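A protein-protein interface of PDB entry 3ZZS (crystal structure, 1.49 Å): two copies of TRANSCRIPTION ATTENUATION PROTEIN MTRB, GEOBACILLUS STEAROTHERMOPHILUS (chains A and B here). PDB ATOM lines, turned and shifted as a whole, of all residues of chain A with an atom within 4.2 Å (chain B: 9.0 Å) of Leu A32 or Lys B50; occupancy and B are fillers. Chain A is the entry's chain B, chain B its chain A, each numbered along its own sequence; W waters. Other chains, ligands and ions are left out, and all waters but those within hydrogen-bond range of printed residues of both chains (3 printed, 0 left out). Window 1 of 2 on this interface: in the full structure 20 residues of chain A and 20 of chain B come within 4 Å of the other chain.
OE2 of Glu A30 is in salt-bridge range of NZ of Lys B50 (2.8 Å). NZ of Lys B50 is in hydrogen-bond range of O of Lys A31, 3.3 Å away. The side-chain carboxylate (OE1) of Glu A36 is in salt-bridge range of the side-chain amino group (NZ) of Lys B50, at 3.9 Å. N of Val B51 is in hydrogen-bond range of O of Val A37. The guanidinium group (NE) of Arg B52 is in salt-bridge range of the side-chain carboxylate (OE2) of Glu A36, 2.9 Å away.
The backbone NH of Ile B16 sits at hydrogen-bond distance from the backbone carbonyl oxygen of Lys B50 (2.8 Å). The backbone NH (N) of Ser B47 sits at hydrogen-bond distance from the backbone carbonyl oxygen (O) of Leu B18 (3.2 Å). N of Ile A6 sits at hydrogen-bond distance from O of Leu A38 (2.8 Å). The backbone carbonyl oxygen of Glu A36 is in hydrogen-bond range of the backbone NH of Ala A8 (3.0 Å). O of Leu A32 is in hydrogen-bond range of N of Gly A12, at 3.2 Å. The backbone NH (N) of Leu A32 lies within hydrogen-bond range of the backbone carbonyl oxygen (O) of Val A13 (2.8 Å).
Glu A30 touches Leu B18. Leu A32 touches Lys B50. Val B51 touches Glu A36 (O to CA, 3.5 Å). Val A37 touches Ile B49. O of Val A37 touches CA of Lys B50, 3.3 Å away. CA of Leu A38 touches O of Ile B49, at 3.5 Å. Lys B50 touches Leu A38 (CB to CD1, 3.9 Å).
Of chain A, only Glu A30, Lys A31, Leu A32, Glu A36, Val A37 and Leu A38 come within 4 Å of Lys B50. No residue of chain B comes within 4 Å of Gly A12. Of the printed residues of chain B, Glu A36 touches Lys B50, Val B51 and Arg B52. Of the printed residues of chain A, Leu B18 touches Glu A30. Printed residues of chain A within 4 Å of Val B51: Glu A36 (3.5 Å) and Val A37 (2.8 Å). Of the printed residues of chain B, Lys A31 touches Lys B50. The nearest printed residue of chain A that does not touch Lys B50 is Asp A33 (5.8 Å). The nearest printed residue of chain A that does not touch Val B51 is Leu A38 (5.0 Å).
Hydrophobic or aromatic side chains of chain B within 4 Å of the printed part of chain A: Leu B18. Along chain B the printed residues that touch a printed residue of chain A span positions 18 to 52. Of the 14 printed residues of chain A, 6 touch a printed residue of chain B. Among the printed residues, Asp or Glu carboxylates within 4 Å of a Lys or Arg side-chain nitrogen of the other chain: Glu A30 with Lys B50, Glu A36 with Lys B50 and Glu A36 with Arg B52.
Positions printed for both chains: 6, 13, 15, 30, 32 and 38.
Water W3 lies within hydrogen-bond range of OE1 of Glu A36, NZ of Lys B50, O of Lys A31 and NH2 of Arg B52. Water W1 bridges OE2 of Glu A36 (2.7 Å) and NE of Arg B52 (2.8 Å). Water W2 lies within hydrogen-bond range of O of Lys A31 (2.9 Å) and NZ of Lys B50 (3.1 Å).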
ATOM      1  N   ILE A   6      36.177 -28.898  26.961  1.00  0.00           N
ATOM      2  CA  ILE A   6      36.400 -30.293  26.614  1.00  0.00           C
ATOM      3  C   ILE A   6      35.415 -30.692  25.528  1.00  0.00           C
ATOM      4  O   ILE A   6      34.205 -30.634  25.739  1.00  0.00           O
ATOM      5  CB  ILE A   6      36.212 -31.220  27.834  1.00  0.00           C
ATOM      6  CG1 ILE A   6      37.165 -30.830  28.970  1.00  0.00           C
ATOM      7  CG2 ILE A   6      36.410 -32.681  27.414  1.00  0.00           C
ATOM      8  CD1 ILE A   6      36.622 -31.027  30.350  1.00  0.00           C
ATOM      9  N   ALA A   8      34.329 -33.940  23.298  1.00  0.00           N
ATOM     10  CA  ALA A   8      34.457 -35.384  23.129  1.00  0.00           C
ATOM     11  C   ALA A   8      34.693 -35.732  21.662  1.00  0.00           C
ATOM     12  O   ALA A   8      33.986 -35.244  20.780  1.00  0.00           O
ATOM     13  CB  ALA A   8      33.216 -36.098  23.649  1.00  0.00           C
ATOM     14  N   GLU A  10      34.869 -39.054  20.830  1.00  0.00           N
ATOM     15  CA  GLU A  10      34.262 -40.378  20.748  1.00  0.00           C
ATOM     16  C   GLU A  10      33.173 -40.447  21.805  1.00  0.00           C
ATOM     17  O   GLU A  10      33.109 -39.587  22.679  1.00  0.00           O
ATOM     18  CB  GLU A  10      35.307 -41.468  20.972  1.00  0.00           C
ATOM     19  CG  GLU A  10      35.877 -41.479  22.378  1.00  0.00           C
ATOM     20  CD  GLU A  10      36.943 -42.534  22.600  1.00  0.00           C
ATOM     21  OE1 GLU A  10      37.217 -43.344  21.687  1.00  0.00           O
ATOM     22  OE2 GLU A  10      37.511 -42.546  23.705  1.00  0.00           O
ATOM     23  N   ASP A  11      32.322 -41.466  21.732  1.00  0.00           N
ATOM     24  CA  ASP A  11      31.301 -41.681  22.748  1.00  0.00           C
ATOM     25  C   ASP A  11      31.921 -42.111  24.075  1.00  0.00           C
ATOM     26  O   ASP A  11      32.977 -42.736  24.103  1.00  0.00           O
ATOM     27  CB  ASP A  11      30.291 -42.743  22.288  1.00  0.00           C
ATOM     28  CG  ASP A  11      29.325 -42.224  21.233  1.00  0.00           C
ATOM     29  OD1 ASP A  11      29.171 -40.993  21.080  1.00  0.00           O
ATOM     30  OD2 ASP A  11      28.689 -43.064  20.571  1.00  0.00           O
ATOM     31  N   GLY A  12      31.259 -41.757  25.172  1.00  0.00           N
ATOM     32  CA  GLY A  12      31.615 -42.270  26.494  1.00  0.00           C
ATOM     33  C   GLY A  12      32.779 -41.568  27.169  1.00  0.00           C
ATOM     34  O   GLY A  12      33.361 -42.103  28.106  1.00  0.00           O
ATOM     35  N   VAL A  13      33.144 -40.383  26.683  1.00  0.00           N
ATOM     36  CA  VAL A  13      34.130 -39.550  27.366  1.00  0.00           C
ATOM     37  C   VAL A  13      33.566 -39.183  28.738  1.00  0.00           C
ATOM     38  O   VAL A  13      32.378 -38.913  28.873  1.00  0.00           O
ATOM     39  CB  VAL A  13      34.493 -38.291  26.530  1.00  0.00           C
ATOM     40  CG1 VAL A  13      35.262 -37.252  27.358  1.00  0.00           C
ATOM     41  CG2 VAL A  13      35.284 -38.681  25.283  1.00  0.00           C
ATOM     42  N   VAL A  15      34.108 -36.677  32.085  1.00  0.00           N
ATOM     43  CA  VAL A  15      34.723 -35.513  32.721  1.00  0.00           C
ATOM     44  C   VAL A  15      34.348 -35.584  34.192  1.00  0.00           C
ATOM     45  O   VAL A  15      33.173 -35.516  34.544  1.00  0.00           O
ATOM     46  CB  VAL A  15      34.274 -34.178  32.094  1.00  0.00           C
ATOM     47  CG1 VAL A  15      34.957 -32.996  32.800  1.00  0.00           C
ATOM     48  CG2 VAL A  15      34.569 -34.155  30.597  1.00  0.00           C
ATOM     49  N   GLU A  30      30.532 -36.434  34.414  1.00  0.00           N
ATOM     50  CA  GLU A  30      29.695 -36.007  33.308  1.00  0.00           C
ATOM     51  C   GLU A  30      30.099 -36.785  32.072  1.00  0.00           C
ATOM     52  O   GLU A  30      31.237 -36.686  31.616  1.00  0.00           O
ATOM     53  CB  GLU A  30      29.834 -34.503  33.058  1.00  0.00           C
ATOM     54  CG  GLU A  30      28.842 -33.943  32.034  1.00  0.00           C
ATOM     55  CD  GLU A  30      27.391 -34.051  32.483  1.00  0.00           C
ATOM     56  OE1 GLU A  30      27.123 -33.986  33.703  1.00  0.00           O
ATOM     57  OE2 GLU A  30      26.510 -34.206  31.613  1.00  0.00           O
ATOM     58  N   LYS A  31      29.171 -37.588  31.551  1.00  0.00           N
ATOM     59  CA  LYS A  31      29.411 -38.358  30.338  1.00  0.00           C
ATOM     60  C   LYS A  31      29.154 -37.484  29.114  1.00  0.00           C
ATOM     61  O   LYS A  31      28.116 -36.820  29.023  1.00  0.00           O
ATOM     62  CB  LYS A  31      28.512 -39.590  30.295  1.00  0.00           C
ATOM     63  CG  LYS A  31      28.829 -40.638  31.345  1.00  0.00           C
ATOM     64  CD  LYS A  31      27.862 -41.807  31.258  1.00  0.00           C
ATOM     65  CE  LYS A  31      28.134 -42.854  32.335  1.00  0.00           C
ATOM     66  NZ  LYS A  31      27.240 -44.037  32.209  1.00  0.00           N
ATOM     67  N   LEU A  32      30.101 -37.482  28.185  1.00  0.00           N
ATOM     68  CA  LEU A  32      29.957 -36.768  26.928  1.00  0.00           C
ATOM     69  C   LEU A  32      29.963 -37.756  25.789  1.00  0.00           C
ATOM     70  O   LEU A  32      30.859 -38.599  25.683  1.00  0.00           O
ATOM     71  CB  LEU A  32      31.104 -35.788  26.707  1.00  0.00           C
ATOM     72  CG  LEU A  32      31.260 -34.631  27.686  1.00  0.00           C
ATOM     73  CD1 LEU A  32      32.481 -33.805  27.274  1.00  0.00           C
ATOM     74  CD2 LEU A  32      30.024 -33.753  27.749  1.00  0.00           C
ATOM     75  N   ASP A  33      28.986 -37.640  24.914  1.00  0.00           N
ATOM     76  CA  ASP A  33      29.040 -38.417  23.695  1.00  0.00           C
ATOM     77  C   ASP A  33      29.724 -37.624  22.601  1.00  0.00           C
ATOM     78  O   ASP A  33      30.010 -36.432  22.768  1.00  0.00           O
ATOM     79  CB  ASP A  33      27.654 -38.919  23.332  1.00  0.00           C
ATOM     80  CG  ASP A  33      27.308 -40.199  24.095  1.00  0.00           C
ATOM     81  OD1 ASP A  33      28.238 -40.867  24.637  1.00  0.00           O
ATOM     82  OD2 ASP A  33      26.125 -40.541  24.160  1.00  0.00           O
ATOM     83  N   GLU A  36      29.947 -33.640  21.728  1.00  0.00           N
ATOM     84  CA  GLU A  36      29.439 -32.777  22.791  1.00  0.00           C
ATOM     85  C   GLU A  36      30.587 -32.006  23.432  1.00  0.00           C
ATOM     86  O   GLU A  36      31.716 -32.475  23.459  1.00  0.00           O
ATOM     87  CB  GLU A  36      28.688 -33.580  23.851  1.00  0.00           C
ATOM     88  CG  GLU A  36      27.428 -34.241  23.308  1.00  0.00           C
ATOM     89  CD  GLU A  36      26.656 -35.051  24.331  1.00  0.00           C
ATOM     90  OE1 GLU A  36      27.200 -35.401  25.392  1.00  0.00           O
ATOM     91  OE2 GLU A  36      25.477 -35.354  24.052  1.00  0.00           O
ATOM     92  N   VAL A  37      30.273 -30.827  23.952  1.00  0.00           N
ATOM     93  CA  VAL A  37      31.262 -29.957  24.575  1.00  0.00           C
ATOM     94  C   VAL A  37      30.824 -29.629  25.997  1.00  0.00           C
ATOM     95  O   VAL A  37      29.659 -29.329  26.251  1.00  0.00           O
ATOM     96  CB  VAL A  37      31.458 -28.651  23.756  1.00  0.00           C
ATOM     97  CG1 VAL A  37      32.363 -27.650  24.490  1.00  0.00           C
ATOM     98  CG2 VAL A  37      32.013 -28.954  22.357  1.00  0.00           C
ATOM     99  N   LEU A  38      31.770 -29.703  26.921  1.00  0.00           N
ATOM    100  CA  LEU A  38      31.572 -29.237  28.277  1.00  0.00           C
ATOM    101  C   LEU A  38      32.560 -28.111  28.540  1.00  0.00           C
ATOM    102  O   LEU A  38      33.769 -28.258  28.301  1.00  0.00           O
ATOM    103  CB  LEU A  38      31.790 -30.354  29.293  1.00  0.00           C
ATOM    104  CG  LEU A  38      31.433 -30.008  30.744  1.00  0.00           C
ATOM    105  CD1 LEU A  38      29.927 -29.762  30.924  1.00  0.00           C
ATOM    106  CD2 LEU A  38      31.929 -31.111  31.690  1.00  0.00           C
ATOM    107  N   VAL B   4      30.487 -17.440  27.226  1.00  0.00           N
ATOM    108  CA  VAL B   4      30.709 -18.220  26.027  1.00  0.00           C
ATOM    109  C   VAL B   4      29.700 -17.795  24.964  1.00  0.00           C
ATOM    110  O   VAL B   4      28.597 -17.353  25.276  1.00  0.00           O
ATOM    111  CB  VAL B   4      30.594 -19.719  26.327  1.00  0.00           C
ATOM    112  CG1 VAL B   4      31.503 -20.099  27.505  1.00  0.00           C
ATOM    113  CG2 VAL B   4      29.157 -20.088  26.626  1.00  0.00           C
ATOM    114  N   ILE B   6      27.703 -19.230  21.667  1.00  0.00           N
ATOM    115  CA  ILE B   6      27.292 -20.462  21.002  1.00  0.00           C
ATOM    116  C   ILE B   6      26.379 -20.146  19.824  1.00  0.00           C
ATOM    117  O   ILE B   6      25.273 -19.627  20.023  1.00  0.00           O
ATOM    118  CB  ILE B   6      26.549 -21.393  21.986  1.00  0.00           C
ATOM    119  CG1 ILE B   6      27.435 -21.694  23.202  1.00  0.00           C
ATOM    120  CG2 ILE B   6      26.092 -22.677  21.278  1.00  0.00           C
ATOM    121  CD1 ILE B   6      26.678 -21.919  24.481  1.00  0.00           C
ATOM    122  N   VAL B  13      19.899 -27.416  18.851  1.00  0.00           N
ATOM    123  CA  VAL B  13      21.101 -27.360  19.679  1.00  0.00           C
ATOM    124  C   VAL B  13      20.654 -27.050  21.104  1.00  0.00           C
ATOM    125  O   VAL B  13      19.790 -26.203  21.306  1.00  0.00           O
ATOM    126  CB  VAL B  13      22.119 -26.333  19.150  1.00  0.00           C
ATOM    127  CG1 VAL B  13      23.237 -26.064  20.170  1.00  0.00           C
ATOM    128  CG2 VAL B  13      22.698 -26.812  17.822  1.00  0.00           C
ATOM    129  N   ASN B  14      21.217 -27.781  22.066  1.00  0.00           N
ATOM    130  CA  ASN B  14      20.828 -27.648  23.450  1.00  0.00           C
ATOM    131  C   ASN B  14      21.994 -27.101  24.257  1.00  0.00           C
ATOM    132  O   ASN B  14      23.082 -27.660  24.246  1.00  0.00           O
ATOM    133  CB  ASN B  14      20.368 -29.008  23.966  1.00  0.00           C
ATOM    134  CG  ASN B  14      19.524 -28.906  25.199  1.00  0.00           C
ATOM    135  OD1 ASN B  14      19.484 -27.866  25.848  1.00  0.00           O
ATOM    136  ND2 ASN B  14      18.837 -29.987  25.535  1.00  0.00           N
ATOM    137  N   VAL B  15      21.759 -25.976  24.926  1.00  0.00           N
ATOM    138  CA  VAL B  15      22.746 -25.375  25.813  1.00  0.00           C
ATOM    139  C   VAL B  15      22.232 -25.606  27.224  1.00  0.00           C
ATOM    140  O   VAL B  15      21.139 -25.147  27.582  1.00  0.00           O
ATOM    141  CB  VAL B  15      22.976 -23.868  25.543  1.00  0.00           C
ATOM    142  CG1 VAL B  15      24.056 -23.338  26.479  1.00  0.00           C
ATOM    143  CG2 VAL B  15      23.351 -23.642  24.073  1.00  0.00           C
ATOM    144  N   ILE B  16      23.026 -26.331  28.006  1.00  0.00           N
ATOM    145  CA  ILE B  16      22.596 -26.895  29.275  1.00  0.00           C
ATOM    146  C   ILE B  16      23.431 -26.324  30.407  1.00  0.00           C
ATOM    147  O   ILE B  16      24.655 -26.474  30.417  1.00  0.00           O
ATOM    148  CB  ILE B  16      22.728 -28.432  29.263  1.00  0.00           C
ATOM    149  CG1 ILE B  16      21.931 -29.044  28.097  1.00  0.00           C
ATOM    150  CG2 ILE B  16      22.273 -29.021  30.591  1.00  0.00           C
ATOM    151  CD1 ILE B  16      22.365 -30.464  27.718  1.00  0.00           C
ATOM    152  N   GLY B  17      22.771 -25.672  31.359  1.00  0.00           N
ATOM    153  CA  GLY B  17      23.456 -25.080  32.493  1.00  0.00           C
ATOM    154  C   GLY B  17      23.509 -26.012  33.688  1.00  0.00           C
ATOM    155  O   GLY B  17      22.483 -26.526  34.132  1.00  0.00           O
ATOM    156  N   LEU B  18      24.712 -26.228  34.211  1.00  0.00           N
ATOM    157  CA  LEU B  18      24.873 -27.218  35.354  1.00  0.00           C
ATOM    158  C   LEU B  18      25.052 -26.408  36.640  1.00  0.00           C
ATOM    159  O   LEU B  18      25.663 -25.339  36.654  1.00  0.00           O
ATOM    160  CB  LEU B  18      26.114 -28.100  35.192  1.00  0.00           C
ATOM    161  CG  LEU B  18      26.047 -29.258  34.195  1.00  0.00           C
ATOM    162  CD1 LEU B  18      26.020 -28.741  32.776  1.00  0.00           C
ATOM    163  CD2 LEU B  18      27.224 -30.203  34.383  1.00  0.00           C
ATOM    164  N   THR B  19      24.397 -26.881  37.695  1.00  0.00           N
ATOM    165  CA  THR B  19      24.356 -26.157  38.961  1.00  0.00           C
ATOM    166  C   THR B  19      25.720 -25.989  39.623  1.00  0.00           C
ATOM    167  O   THR B  19      26.482 -26.941  39.756  1.00  0.00           O
ATOM    168  CB  THR B  19      23.452 -26.870  39.986  1.00  0.00           C
ATOM    169  OG1 THR B  19      23.896 -28.229  40.162  1.00  0.00           O
ATOM    170  CG2 THR B  19      21.988 -26.844  39.530  1.00  0.00           C
ATOM    171  N   PHE B  26      21.460 -30.583  35.873  1.00  0.00           N
ATOM    172  CA  PHE B  26      21.110 -29.526  34.973  1.00  0.00           C
ATOM    173  C   PHE B  26      19.955 -28.748  35.553  1.00  0.00           C
ATOM    174  O   PHE B  26      19.078 -29.322  36.085  1.00  0.00           O
ATOM    175  CB  PHE B  26      20.809 -30.076  33.557  1.00  0.00           C
ATOM    176  CG  PHE B  26      19.354 -30.295  33.268  1.00  0.00           C
ATOM    177  CD1 PHE B  26      18.562 -29.291  32.742  1.00  0.00           C
ATOM    178  CD2 PHE B  26      18.789 -31.517  33.501  1.00  0.00           C
ATOM    179  CE1 PHE B  26      17.212 -29.511  32.510  1.00  0.00           C
ATOM    180  CE2 PHE B  26      17.458 -31.711  33.253  1.00  0.00           C
ATOM    181  CZ  PHE B  26      16.699 -30.704  32.777  1.00  0.00           C
ATOM    182  N   HIS B  28      18.798 -25.789  33.683  1.00  0.00           N
ATOM    183  CA  HIS B  28      18.163 -25.153  32.543  1.00  0.00           C
ATOM    184  C   HIS B  28      18.699 -25.719  31.238  1.00  0.00           C
ATOM    185  O   HIS B  28      19.906 -25.942  31.099  1.00  0.00           O
ATOM    186  CB  HIS B  28      18.387 -23.636  32.546  1.00  0.00           C
ATOM    187  CG  HIS B  28      17.619 -22.938  31.471  1.00  0.00           C
ATOM    188  ND1 HIS B  28      16.254 -22.761  31.539  1.00  0.00           N
ATOM    189  CD2 HIS B  28      18.005 -22.454  30.266  1.00  0.00           C
ATOM    190  CE1 HIS B  28      15.837 -22.163  30.438  1.00  0.00           C
ATOM    191  NE2 HIS B  28      16.879 -21.977  29.644  1.00  0.00           N
ATOM    192  N   SER B  29      17.779 -25.933  30.295  1.00  0.00           N
ATOM    193  CA  SER B  29      18.082 -26.325  28.927  1.00  0.00           C
ATOM    194  C   SER B  29      17.538 -25.251  27.989  1.00  0.00           C
ATOM    195  O   SER B  29      16.325 -25.035  27.950  1.00  0.00           O
ATOM    196  CB  SER B  29      17.437 -27.674  28.635  1.00  0.00           C
ATOM    197  OG  SER B  29      17.489 -28.004  27.259  1.00  0.00           O
ATOM    198  N   GLU B  30      18.417 -24.572  27.256  1.00  0.00           N
ATOM    199  CA  GLU B  30      18.008 -23.589  26.260  1.00  0.00           C
ATOM    200  C   GLU B  30      18.270 -24.125  24.864  1.00  0.00           C
ATOM    201  O   GLU B  30      19.401 -24.448  24.524  1.00  0.00           O
ATOM    202  CB  GLU B  30      18.756 -22.265  26.447  1.00  0.00           C
ATOM    203  CG  GLU B  30      18.210 -21.127  25.582  1.00  0.00           C
ATOM    204  CD  GLU B  30      16.786 -20.739  25.956  1.00  0.00           C
ATOM    205  OE1 GLU B  30      16.426 -20.864  27.144  1.00  0.00           O
ATOM    206  OE2 GLU B  30      16.018 -20.301  25.052  1.00  0.00           O
ATOM    207  N   LEU B  32      18.387 -23.824  20.727  1.00  0.00           N
ATOM    208  CA  LEU B  32      18.693 -22.884  19.657  1.00  0.00           C
ATOM    209  C   LEU B  32      18.357 -23.512  18.318  1.00  0.00           C
ATOM    210  O   LEU B  32      18.751 -24.655  18.055  1.00  0.00           O
ATOM    211  CB  LEU B  32      20.182 -22.541  19.650  1.00  0.00           C
ATOM    212  CG  LEU B  32      20.753 -21.800  20.851  1.00  0.00           C
ATOM    213  CD1 LEU B  32      22.277 -21.823  20.802  1.00  0.00           C
ATOM    214  CD2 LEU B  32      20.220 -20.377  20.875  1.00  0.00           C
ATOM    215  N   LEU B  38      23.429 -17.937  21.400  1.00  0.00           N
ATOM    216  CA  LEU B  38      23.291 -17.678  22.827  1.00  0.00           C
ATOM    217  C   LEU B  38      24.635 -17.216  23.353  1.00  0.00           C
ATOM    218  O   LEU B  38      25.659 -17.863  23.109  1.00  0.00           O
ATOM    219  CB  LEU B  38      22.832 -18.924  23.598  1.00  0.00           C
ATOM    220  CG  LEU B  38      22.453 -18.675  25.063  1.00  0.00           C
ATOM    221  CD1 LEU B  38      21.170 -17.856  25.174  1.00  0.00           C
ATOM    222  CD2 LEU B  38      22.310 -19.991  25.814  1.00  0.00           C
ATOM    223  N   PHE B  42      29.058 -17.589  32.900  1.00  0.00           N
ATOM    224  CA  PHE B  42      29.137 -18.308  34.155  1.00  0.00           C
ATOM    225  C   PHE B  42      28.628 -17.374  35.248  1.00  0.00           C
ATOM    226  O   PHE B  42      28.844 -16.172  35.189  1.00  0.00           O
ATOM    227  CB  PHE B  42      30.558 -18.772  34.426  1.00  0.00           C
ATOM    228  CG  PHE B  42      31.008 -19.851  33.497  1.00  0.00           C
ATOM    229  CD1 PHE B  42      30.440 -21.120  33.582  1.00  0.00           C
ATOM    230  CD2 PHE B  42      31.956 -19.617  32.526  1.00  0.00           C
ATOM    231  CE1 PHE B  42      30.806 -22.121  32.747  1.00  0.00           C
ATOM    232  CE2 PHE B  42      32.331 -20.638  31.667  1.00  0.00           C
ATOM    233  CZ  PHE B  42      31.752 -21.888  31.785  1.00  0.00           C
ATOM    234  N   THR B  46      25.403 -21.143  37.691  1.00  0.00           N
ATOM    235  CA  THR B  46      25.899 -21.951  36.584  1.00  0.00           C
ATOM    236  C   THR B  46      27.426 -21.962  36.576  1.00  0.00           C
ATOM    237  O   THR B  46      28.053 -20.934  36.290  1.00  0.00           O
ATOM    238  CB  THR B  46      25.401 -21.413  35.230  1.00  0.00           C
ATOM    239  OG1 THR B  46      23.966 -21.392  35.224  1.00  0.00           O
ATOM    240  CG2 THR B  46      25.914 -22.275  34.087  1.00  0.00           C
ATOM    241  N   SER B  47      28.018 -23.119  36.886  1.00  0.00           N
ATOM    242  CA  SER B  47      29.479 -23.264  36.891  1.00  0.00           C
ATOM    243  C   SER B  47      30.018 -24.219  35.826  1.00  0.00           C
ATOM    244  O   SER B  47      31.233 -24.423  35.742  1.00  0.00           O
ATOM    245  CB  SER B  47      29.953 -23.720  38.273  1.00  0.00           C
ATOM    246  OG  SER B  47      29.435 -25.004  38.559  1.00  0.00           O
ATOM    247  N   ALA B  48      29.127 -24.794  35.022  1.00  0.00           N
ATOM    248  CA  ALA B  48      29.515 -25.589  33.861  1.00  0.00           C
ATOM    249  C   ALA B  48      28.392 -25.524  32.844  1.00  0.00           C
ATOM    250  O   ALA B  48      27.221 -25.442  33.221  1.00  0.00           O
ATOM    251  CB  ALA B  48      29.828 -27.032  34.249  1.00  0.00           C
ATOM    252  N   ILE B  49      28.763 -25.552  31.566  1.00  0.00           N
ATOM    253  CA  ILE B  49      27.818 -25.453  30.459  1.00  0.00           C
ATOM    254  C   ILE B  49      28.113 -26.596  29.503  1.00  0.00           C
ATOM    255  O   ILE B  49      29.254 -26.771  29.081  1.00  0.00           O
ATOM    256  CB  ILE B  49      27.932 -24.095  29.731  1.00  0.00           C
ATOM    257  CG1 ILE B  49      27.573 -22.955  30.690  1.00  0.00           C
ATOM    258  CG2 ILE B  49      27.051 -24.056  28.470  1.00  0.00           C
ATOM    259  CD1 ILE B  49      27.956 -21.557  30.225  1.00  0.00           C
ATOM    260  N   LYS B  50      27.080 -27.356  29.161  1.00  0.00           N
ATOM    261  CA  LYS B  50      27.185 -28.447  28.207  1.00  0.00           C
ATOM    262  C   LYS B  50      26.456 -28.060  26.931  1.00  0.00           C
ATOM    263  O   LYS B  50      25.347 -27.526  26.986  1.00  0.00           O
ATOM    264  CB  LYS B  50      26.606 -29.719  28.820  1.00  0.00           C
ATOM    265  CG  LYS B  50      26.754 -30.965  27.973  1.00  0.00           C
ATOM    266  CD  LYS B  50      26.256 -32.165  28.764  1.00  0.00           C
ATOM    267  CE  LYS B  50      26.390 -33.467  28.052  1.00  0.00           C
ATOM    268  NZ  LYS B  50      25.799 -34.531  28.925  1.00  0.00           N
ATOM    269  N   VAL B  51      27.091 -28.309  25.788  1.00  0.00           N
ATOM    270  CA  VAL B  51      26.491 -28.039  24.488  1.00  0.00           C
ATOM    271  C   VAL B  51      26.342 -29.340  23.710  1.00  0.00           C
ATOM    272  O   VAL B  51      27.307 -30.082  23.525  1.00  0.00           O
ATOM    273  CB  VAL B  51      27.309 -27.013  23.682  1.00  0.00           C
ATOM    274  CG1 VAL B  51      26.605 -26.675  22.367  1.00  0.00           C
ATOM    275  CG2 VAL B  51      27.540 -25.745  24.518  1.00  0.00           C
ATOM    276  N   ARG B  52      25.106 -29.616  23.297  1.00  0.00           N
ATOM    277  CA  ARG B  52      24.763 -30.786  22.506  1.00  0.00           C
ATOM    278  C   ARG B  52      24.188 -30.298  21.187  1.00  0.00           C
ATOM    279  O   ARG B  52      23.328 -29.423  21.159  1.00  0.00           O
ATOM    280  CB  ARG B  52      23.763 -31.671  23.272  1.00  0.00           C
ATOM    281  CG  ARG B  52      23.352 -32.951  22.580  1.00  0.00           C
ATOM    282  CD  ARG B  52      22.279 -33.670  23.391  1.00  0.00           C
ATOM    283  NE  ARG B  52      22.830 -34.309  24.585  1.00  0.00           N
ATOM    284  CZ  ARG B  52      22.144 -34.628  25.684  1.00  0.00           C
ATOM    285  NH1 ARG B  52      20.851 -34.329  25.812  1.00  0.00           N
ATOM    286  NH2 ARG B  52      22.774 -35.230  26.684  1.00  0.00           N
ATOM    287  N   GLY B  53      24.667 -30.869  20.096  1.00  0.00           N
ATOM    288  CA  GLY B  53      24.260 -30.442  18.769  1.00  0.00           C
ATOM    289  C   GLY B  53      25.408 -29.746  18.071  1.00  0.00           C
ATOM    290  O   GLY B  53      26.388 -29.337  18.704  1.00  0.00           O
ATOM    291  N   ALA B  55      27.405 -26.983  16.620  1.00  0.00           N
ATOM    292  CA  ALA B  55      27.488 -25.586  17.000  1.00  0.00           C
ATOM    293  C   ALA B  55      28.896 -25.048  16.772  1.00  0.00           C
ATOM    294  O   ALA B  55      29.857 -25.810  16.681  1.00  0.00           O
ATOM    295  CB  ALA B  55      27.081 -25.425  18.459  1.00  0.00           C
ATOM    296  N   ILE B  57      31.450 -22.389  18.616  1.00  0.00           N
ATOM    297  CA  ILE B  57      31.578 -21.833  19.967  1.00  0.00           C
ATOM    298  C   ILE B  57      32.826 -20.967  20.084  1.00  0.00           C
ATOM    299  O   ILE B  57      33.892 -21.346  19.595  1.00  0.00           O
ATOM    300  CB  ILE B  57      31.619 -22.959  21.022  1.00  0.00           C
ATOM    301  CG1 ILE B  57      30.349 -23.816  20.966  1.00  0.00           C
ATOM    302  CG2 ILE B  57      31.819 -22.392  22.436  1.00  0.00           C
ATOM    303  CD1 ILE B  57      30.442 -25.099  21.753  1.00  0.00           C
HETATM  304  O   HOH W   1      23.327 -36.664  23.149  1.00  0.00           O
HETATM  305  O   HOH W   2      25.336 -37.432  29.760  1.00  0.00           O
HETATM  306  O   HOH W   3      25.601 -36.583  27.144  1.00  0.00           O
